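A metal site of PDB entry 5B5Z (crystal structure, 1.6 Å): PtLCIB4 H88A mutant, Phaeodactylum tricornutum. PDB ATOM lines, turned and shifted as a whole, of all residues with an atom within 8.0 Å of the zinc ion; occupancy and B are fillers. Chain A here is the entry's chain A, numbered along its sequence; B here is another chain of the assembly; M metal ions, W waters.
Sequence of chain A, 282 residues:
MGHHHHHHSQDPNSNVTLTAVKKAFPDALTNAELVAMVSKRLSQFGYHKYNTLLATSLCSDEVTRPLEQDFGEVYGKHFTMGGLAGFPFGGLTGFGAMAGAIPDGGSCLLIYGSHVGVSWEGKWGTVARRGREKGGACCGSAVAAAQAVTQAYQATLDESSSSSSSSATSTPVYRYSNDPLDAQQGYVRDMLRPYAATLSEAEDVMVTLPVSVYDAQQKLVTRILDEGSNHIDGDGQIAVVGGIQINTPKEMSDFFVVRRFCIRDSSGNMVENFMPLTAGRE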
ATOM      1  N   LEU A  58      19.527 -12.471 -12.765  1.00  0.00           N
ATOM      2  CA  LEU A  58      20.989 -12.400 -12.730  1.00  0.00           C
ATOM      3  C   LEU A  58      21.448 -11.142 -13.461  1.00  0.00           C
ATOM      4  O   LEU A  58      20.666 -10.539 -14.215  1.00  0.00           O
ATOM      5  CB  LEU A  58      21.600 -13.649 -13.372  1.00  0.00           C
ATOM      6  CG  LEU A  58      21.189 -14.981 -12.724  1.00  0.00           C
ATOM      7  CD1 LEU A  58      21.601 -16.203 -13.589  1.00  0.00           C
ATOM      8  CD2 LEU A  58      21.774 -15.106 -11.315  1.00  0.00           C
ATOM      9  N   CYS A  59      22.694 -10.740 -13.258  1.00  0.00           N
ATOM     10  CA  CYS A  59      23.175  -9.498 -13.888  1.00  0.00           C
ATOM     11  C   CYS A  59      23.185  -9.624 -15.411  1.00  0.00           C
ATOM     12  O   CYS A  59      23.396 -10.713 -15.985  1.00  0.00           O
ATOM     13  CB  CYS A  59      24.599  -9.140 -13.389  1.00  0.00           C
ATOM     14  SG  CYS A  59      25.180  -7.525 -13.993  1.00  0.00           S
ATOM     15  N   SER A  60      22.954  -8.491 -16.060  1.00  0.00           N
ATOM     16  CA  SER A  60      22.950  -8.417 -17.515  1.00  0.00           C
ATOM     17  C   SER A  60      24.327  -8.704 -18.127  1.00  0.00           C
ATOM     18  O   SER A  60      24.420  -9.000 -19.310  1.00  0.00           O
ATOM     19  CB  SER A  60      22.451  -7.032 -17.902  1.00  0.00           C
ATOM     20  OG  SER A  60      23.043  -6.061 -17.082  1.00  0.00           O
ATOM     21  N   ASP A  61      25.382  -8.594 -17.326  1.00  0.00           N
ATOM     22  CA  ASP A  61      26.752  -8.939 -17.745  1.00  0.00           C
ATOM     23  C   ASP A  61      26.841 -10.306 -18.477  1.00  0.00           C
ATOM     24  O   ASP A  61      26.253 -11.290 -18.028  1.00  0.00           O
ATOM     25  CB  ASP A  61      27.630  -8.943 -16.487  1.00  0.00           C
ATOM     26  CG  ASP A  61      29.128  -8.911 -16.782  1.00  0.00           C
ATOM     27  OD1 ASP A  61      29.573  -9.463 -17.821  1.00  0.00           O
ATOM     28  OD2 ASP A  61      29.866  -8.370 -15.910  1.00  0.00           O
ATOM     29  N   GLU A  62      27.565 -10.350 -19.600  1.00  0.00           N
ATOM     30  CA  GLU A  62      27.709 -11.601 -20.368  1.00  0.00           C
ATOM     31  C   GLU A  62      28.291 -12.746 -19.541  1.00  0.00           C
ATOM     32  O   GLU A  62      28.027 -13.908 -19.812  1.00  0.00           O
ATOM     33  CB  GLU A  62      28.587 -11.390 -21.615  1.00  0.00           C
ATOM     34  CG  GLU A  62      30.012 -10.891 -21.332  1.00  0.00           C
ATOM     35  CD  GLU A  62      31.015 -11.996 -21.025  1.00  0.00           C
ATOM     36  OE1 GLU A  62      32.153 -11.675 -20.619  1.00  0.00           O
ATOM     37  OE2 GLU A  62      30.688 -13.193 -21.213  1.00  0.00           O
ATOM     38  N   VAL A  63      29.080 -12.431 -18.514  1.00  0.00           N
ATOM     39  CA  VAL A  63      29.721 -13.495 -17.746  1.00  0.00           C
ATOM     40  C   VAL A  63      28.739 -14.324 -16.916  1.00  0.00           C
ATOM     41  O   VAL A  63      29.103 -15.384 -16.397  1.00  0.00           O
ATOM     42  CB  VAL A  63      30.831 -12.952 -16.784  1.00  0.00           C
ATOM     43  CG1 VAL A  63      31.911 -12.272 -17.590  1.00  0.00           C
ATOM     44  CG2 VAL A  63      30.246 -12.024 -15.726  1.00  0.00           C
ATOM     45  N   THR A  64      27.492 -13.882 -16.793  1.00  0.00           N
ATOM     46  CA  THR A  64      26.540 -14.628 -15.980  1.00  0.00           C
ATOM     47  C   THR A  64      25.796 -15.674 -16.818  1.00  0.00           C
ATOM     48  O   THR A  64      25.131 -16.552 -16.268  1.00  0.00           O
ATOM     49  CB  THR A  64      25.529 -13.689 -15.277  1.00  0.00           C
ATOM     50  OG1 THR A  64      24.697 -13.079 -16.259  1.00  0.00           O
ATOM     51  CG2 THR A  64      26.242 -12.596 -14.472  1.00  0.00           C
ATOM     52  N   GLY A  83      18.623  -7.617 -14.475  1.00  0.00           N
ATOM     53  CA  GLY A  83      19.014  -6.312 -14.969  1.00  0.00           C
ATOM     54  C   GLY A  83      20.346  -6.034 -14.310  1.00  0.00           C
ATOM     55  O   GLY A  83      20.960  -6.961 -13.844  1.00  0.00           O
ATOM     56  N   LEU A  84      20.737  -4.773 -14.215  1.00  0.00           N
ATOM     57  CA  LEU A  84      22.039  -4.454 -13.632  1.00  0.00           C
ATOM     58  C   LEU A  84      22.204  -5.016 -12.219  1.00  0.00           C
ATOM     59  O   LEU A  84      21.311  -4.898 -11.382  1.00  0.00           O
ATOM     60  CB  LEU A  84      22.240  -2.932 -13.625  1.00  0.00           C
ATOM     61  CG  LEU A  84      22.354  -2.308 -15.019  1.00  0.00           C
ATOM     62  CD1 LEU A  84      22.465  -0.808 -14.888  1.00  0.00           C
ATOM     63  CD2 LEU A  84      23.536  -2.894 -15.779  1.00  0.00           C
ATOM     64  N   ALA A  85      23.346  -5.645 -11.976  1.00  0.00           N
ATOM     65  CA  ALA A  85      23.714  -6.258 -10.693  1.00  0.00           C
ATOM     66  C   ALA A  85      22.854  -7.466 -10.294  1.00  0.00           C
ATOM     67  O   ALA A  85      23.069  -8.043  -9.234  1.00  0.00           O
ATOM     68  CB  ALA A  85      23.693  -5.219  -9.586  1.00  0.00           C
ATOM     69  N   GLY A  86      21.904  -7.842 -11.149  1.00  0.00           N
ATOM     70  CA  GLY A  86      21.052  -9.007 -10.890  1.00  0.00           C
ATOM     71  C   GLY A  86      19.760  -8.745 -10.126  1.00  0.00           C
ATOM     72  O   GLY A  86      19.029  -9.675  -9.811  1.00  0.00           O
ATOM     73  N   GLY A 113      20.680 -14.036  -8.021  1.00  0.00           N
ATOM     74  CA  GLY A 113      21.875 -13.791  -7.251  1.00  0.00           C
ATOM     75  C   GLY A 113      22.645 -12.598  -7.719  1.00  0.00           C
ATOM     76  O   GLY A 113      22.485 -12.094  -8.827  1.00  0.00           O
ATOM     77  N   SER A 114      23.542 -12.173  -6.834  1.00  0.00           N
ATOM     78  CA  SER A 114      24.573 -11.250  -7.214  1.00  0.00           C
ATOM     79  C   SER A 114      25.689 -12.018  -7.909  1.00  0.00           C
ATOM     80  O   SER A 114      25.642 -13.228  -8.004  1.00  0.00           O
ATOM     81  CB  SER A 114      25.134 -10.563  -5.974  1.00  0.00           C
ATOM     82  OG  SER A 114      25.694 -11.540  -5.103  1.00  0.00           O
ATOM     83  N   HIS A 115      26.685 -11.319  -8.410  1.00  0.00           N
ATOM     84  CA  HIS A 115      27.861 -12.038  -8.905  1.00  0.00           C
ATOM     85  C   HIS A 115      29.140 -11.241  -8.651  1.00  0.00           C
ATOM     86  O   HIS A 115      29.102 -10.054  -8.338  1.00  0.00           O
ATOM     87  CB  HIS A 115      27.720 -12.391 -10.400  1.00  0.00           C
ATOM     88  CG  HIS A 115      27.926 -11.246 -11.338  1.00  0.00           C
ATOM     89  ND1 HIS A 115      28.912 -11.228 -12.298  1.00  0.00           N
ATOM     90  CD2 HIS A 115      27.252 -10.073 -11.463  1.00  0.00           C
ATOM     91  CE1 HIS A 115      28.847 -10.080 -12.964  1.00  0.00           C
ATOM     92  NE2 HIS A 115      27.837  -9.378 -12.490  1.00  0.00           N
ATOM     93  N   VAL A 116      30.263 -11.924  -8.800  1.00  0.00           N
ATOM     94  CA  VAL A 116      31.569 -11.303  -8.553  1.00  0.00           C
ATOM     95  C   VAL A 116      32.630 -12.065  -9.320  1.00  0.00           C
ATOM     96  O   VAL A 116      32.568 -13.299  -9.391  1.00  0.00           O
ATOM     97  CB  VAL A 116      31.893 -11.270  -7.041  1.00  0.00           C
ATOM     98  CG1 VAL A 116      31.912 -12.675  -6.451  1.00  0.00           C
ATOM     99  CG2 VAL A 116      33.200 -10.536  -6.808  1.00  0.00           C
ATOM    100  N   ARG A 129      38.383 -11.033 -19.362  1.00  0.00           N
ATOM    101  CA  ARG A 129      37.335 -11.087 -20.370  1.00  0.00           C
ATOM    102  C   ARG A 129      37.909 -11.413 -21.750  1.00  0.00           C
ATOM    103  O   ARG A 129      39.017 -10.986 -22.077  1.00  0.00           O
ATOM    104  CB  ARG A 129      36.564  -9.773 -20.412  1.00  0.00           C
ATOM    105  CG  ARG A 129      35.733  -9.516 -19.157  1.00  0.00           C
ATOM    106  CD  ARG A 129      34.917  -8.242 -19.287  1.00  0.00           C
ATOM    107  NE  ARG A 129      34.286  -7.890 -18.002  1.00  0.00           N
ATOM    108  CZ  ARG A 129      33.049  -8.229 -17.664  1.00  0.00           C
ATOM    109  NH1 ARG A 129      32.295  -8.908 -18.512  1.00  0.00           N
ATOM    110  NH2 ARG A 129      32.560  -7.877 -16.487  1.00  0.00           N
ATOM    111  N   ALA A 137      35.928  -4.168 -13.930  1.00  0.00           N
ATOM    112  CA  ALA A 137      35.181  -4.581 -12.751  1.00  0.00           C
ATOM    113  C   ALA A 137      34.166  -5.675 -13.049  1.00  0.00           C
ATOM    114  O   ALA A 137      33.599  -5.746 -14.142  1.00  0.00           O
ATOM    115  CB  ALA A 137      34.491  -3.386 -12.138  1.00  0.00           C
ATOM    116  N   CYS A 138      33.929  -6.522 -12.055  1.00  0.00           N
ATOM    117  CA  CYS A 138      32.925  -7.580 -12.122  1.00  0.00           C
ATOM    118  C   CYS A 138      32.487  -7.880 -10.695  1.00  0.00           C
ATOM    119  O   CYS A 138      33.242  -8.476  -9.942  1.00  0.00           O
ATOM    120  CB  CYS A 138      33.522  -8.829 -12.793  1.00  0.00           C
ATOM    121  SG  CYS A 138      32.383 -10.190 -13.079  1.00  0.00           S
ATOM    122  N   CYS A 139      31.294  -7.479 -10.269  1.00  0.00           N
ATOM    123  CA  CYS A 139      30.236  -6.842 -11.033  1.00  0.00           C
ATOM    124  C   CYS A 139      30.438  -5.339 -11.266  1.00  0.00           C
ATOM    125  O   CYS A 139      30.476  -4.587 -10.324  1.00  0.00           O
ATOM    126  CB  CYS A 139      28.934  -7.100 -10.263  1.00  0.00           C
ATOM    127  SG  CYS A 139      27.446  -6.342 -11.004  1.00  0.00           S
ATOM    128  N   GLY A 140      30.528  -4.901 -12.523  1.00  0.00           N
ATOM    129  CA  GLY A 140      30.716  -3.486 -12.823  1.00  0.00           C
ATOM    130  C   GLY A 140      29.690  -2.553 -12.205  1.00  0.00           C
ATOM    131  O   GLY A 140      30.021  -1.517 -11.613  1.00  0.00           O
ATOM    132  N   SER A 141      28.424  -2.912 -12.356  1.00  0.00           N
ATOM    133  CA  SER A 141      27.332  -2.127 -11.806  1.00  0.00           C
ATOM    134  C   SER A 141      27.421  -1.987 -10.292  1.00  0.00           C
ATOM    135  O   SER A 141      27.306  -0.897  -9.754  1.00  0.00           O
ATOM    136  CB  SER A 141      25.978  -2.753 -12.202  1.00  0.00           C
ATOM    137  OG  SER A 141      24.924  -2.182 -11.441  1.00  0.00           O
ATOM    138  N   ALA A 142      27.611  -3.104  -9.602  1.00  0.00           N
ATOM    139  CA  ALA A 142      27.681  -3.069  -8.139  1.00  0.00           C
ATOM    140  C   ALA A 142      28.892  -2.259  -7.665  1.00  0.00           C
ATOM    141  O   ALA A 142      28.801  -1.519  -6.686  1.00  0.00           O
ATOM    142  CB  ALA A 142      27.723  -4.474  -7.570  1.00  0.00           C
ATOM    143  N   VAL A 143      30.020  -2.412  -8.342  1.00  0.00           N
ATOM    144  CA  VAL A 143      31.243  -1.726  -7.924  1.00  0.00           C
ATOM    145  C   VAL A 143      31.092  -0.220  -8.071  1.00  0.00           C
ATOM    146  O   VAL A 143      31.456   0.543  -7.160  1.00  0.00           O
ATOM    147  CB  VAL A 143      32.472  -2.224  -8.717  1.00  0.00           C
ATOM    148  CG1 VAL A 143      33.664  -1.293  -8.499  1.00  0.00           C
ATOM    149  CG2 VAL A 143      32.844  -3.642  -8.283  1.00  0.00           C
ATOM    150  N   GLN A 245      26.909 -15.730  -7.421  1.00  0.00           N
ATOM    151  CA  GLN A 245      27.539 -16.315  -8.571  1.00  0.00           C
ATOM    152  C   GLN A 245      29.007 -15.879  -8.615  1.00  0.00           C
ATOM    153  O   GLN A 245      29.302 -14.678  -8.548  1.00  0.00           O
ATOM    154  CB  GLN A 245      26.756 -15.876  -9.817  1.00  0.00           C
ATOM    155  CG  GLN A 245      27.267 -16.293 -11.137  1.00  0.00           C
ATOM    156  CD  GLN A 245      26.299 -15.901 -12.242  1.00  0.00           C
ATOM    157  OE1 GLN A 245      25.468 -14.973 -12.073  1.00  0.00           O
ATOM    158  NE2 GLN A 245      26.387 -16.584 -13.363  1.00  0.00           N
ATOM    159  N   ASN A 247      32.318 -15.745 -10.824  1.00  0.00           N
ATOM    160  CA  ASN A 247      32.808 -15.869 -12.193  1.00  0.00           C
ATOM    161  C   ASN A 247      34.323 -15.985 -12.207  1.00  0.00           C
ATOM    162  O   ASN A 247      35.038 -15.066 -11.787  1.00  0.00           O
ATOM    163  CB  ASN A 247      32.341 -14.683 -13.026  1.00  0.00           C
ATOM    164  CG  ASN A 247      30.833 -14.537 -13.002  1.00  0.00           C
ATOM    165  OD1 ASN A 247      30.305 -13.499 -12.620  1.00  0.00           O
ATOM    166  ND2 ASN A 247      30.139 -15.591 -13.363  1.00  0.00           N
ATOM    167  N   PHE B  79      25.631  -9.903 -23.799  1.00  0.00           N
ATOM    168  CA  PHE B  79      25.183  -8.936 -22.796  1.00  0.00           C
ATOM    169  C   PHE B  79      23.697  -8.711 -23.017  1.00  0.00           C
ATOM    170  O   PHE B  79      23.229  -8.638 -24.157  1.00  0.00           O
ATOM    171  CB  PHE B  79      25.987  -7.641 -22.949  1.00  0.00           C
ATOM    172  CG  PHE B  79      25.758  -6.640 -21.859  1.00  0.00           C
ATOM    173  CD1 PHE B  79      24.697  -5.750 -21.920  1.00  0.00           C
ATOM    174  CD2 PHE B  79      26.661  -6.549 -20.791  1.00  0.00           C
ATOM    175  CE1 PHE B  79      24.484  -4.807 -20.922  1.00  0.00           C
ATOM    176  CE2 PHE B  79      26.455  -5.608 -19.786  1.00  0.00           C
ATOM    177  CZ  PHE B  79      25.366  -4.741 -19.851  1.00  0.00           C
ATOM    178  N   ALA B  97      28.817  -0.758 -19.649  1.00  0.00           N
ATOM    179  CA  ALA B  97      29.308  -2.059 -19.187  1.00  0.00           C
ATOM    180  C   ALA B  97      29.631  -2.941 -20.378  1.00  0.00           C
ATOM    181  O   ALA B  97      30.667  -3.610 -20.444  1.00  0.00           O
ATOM    182  CB  ALA B  97      28.285  -2.732 -18.282  1.00  0.00           C
HETATM  183 ZN    ZN M   1      27.214  -7.463 -13.004  1.00  0.00          ZN
HETATM  184  O   HOH W   1      28.662  -6.891 -14.119  1.00  0.00           O
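SG of Cys 138 sits close to ND1 of His 115 (3.7 Å).
The side-chain amide oxygen of Asn 247 sits at hydrogen-bond distance from a ring nitrogen (ND1) of His 115 (2.7 Å).
The backbone NH (N) of Asp 61 sits close to the side-chain sulfur (SG) of Cys 59 (3.5 Å).
The backbone NH (N) of Ala 85 lies close to the side-chain sulfur (SG) of Cys 59 (3.3 Å).
OG1 of Thr 64 sits at hydrogen-bond distance from O of Cys 59, at 2.7 Å.
The backbone carbonyl oxygen of Asp 61 lies within hydrogen-bond range of the side-chain hydroxyl of Thr 64 (3.0 Å).
N of Val 63 lies close to OD1 of Asp 61, 3.1 Å away.
The side-chain carboxylate (OD2) of Asp 61 lies within salt-bridge range of the guanidinium group (NH2) of Arg 129.
Asp 61 touches the zinc ion.
Within 4 Å of the zinc ion: Cys 59, Asp 61, His 115 and Cys 139.
Water W1 is bound to the zinc ion.
The zinc ion is bound by NE2 of His 115.
The zinc ion is bound by SG of Cys 59 (2.3 Å).
SG of Cys 139 is bound to the zinc ion, 2.3 Å away.
The zinc ion has four donor atoms within binding distance.
Water W1 bridges the side-chain carboxylate of Asp 61 (2.6 Å) and the backbone NH of Gly 140 (3.2 Å).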
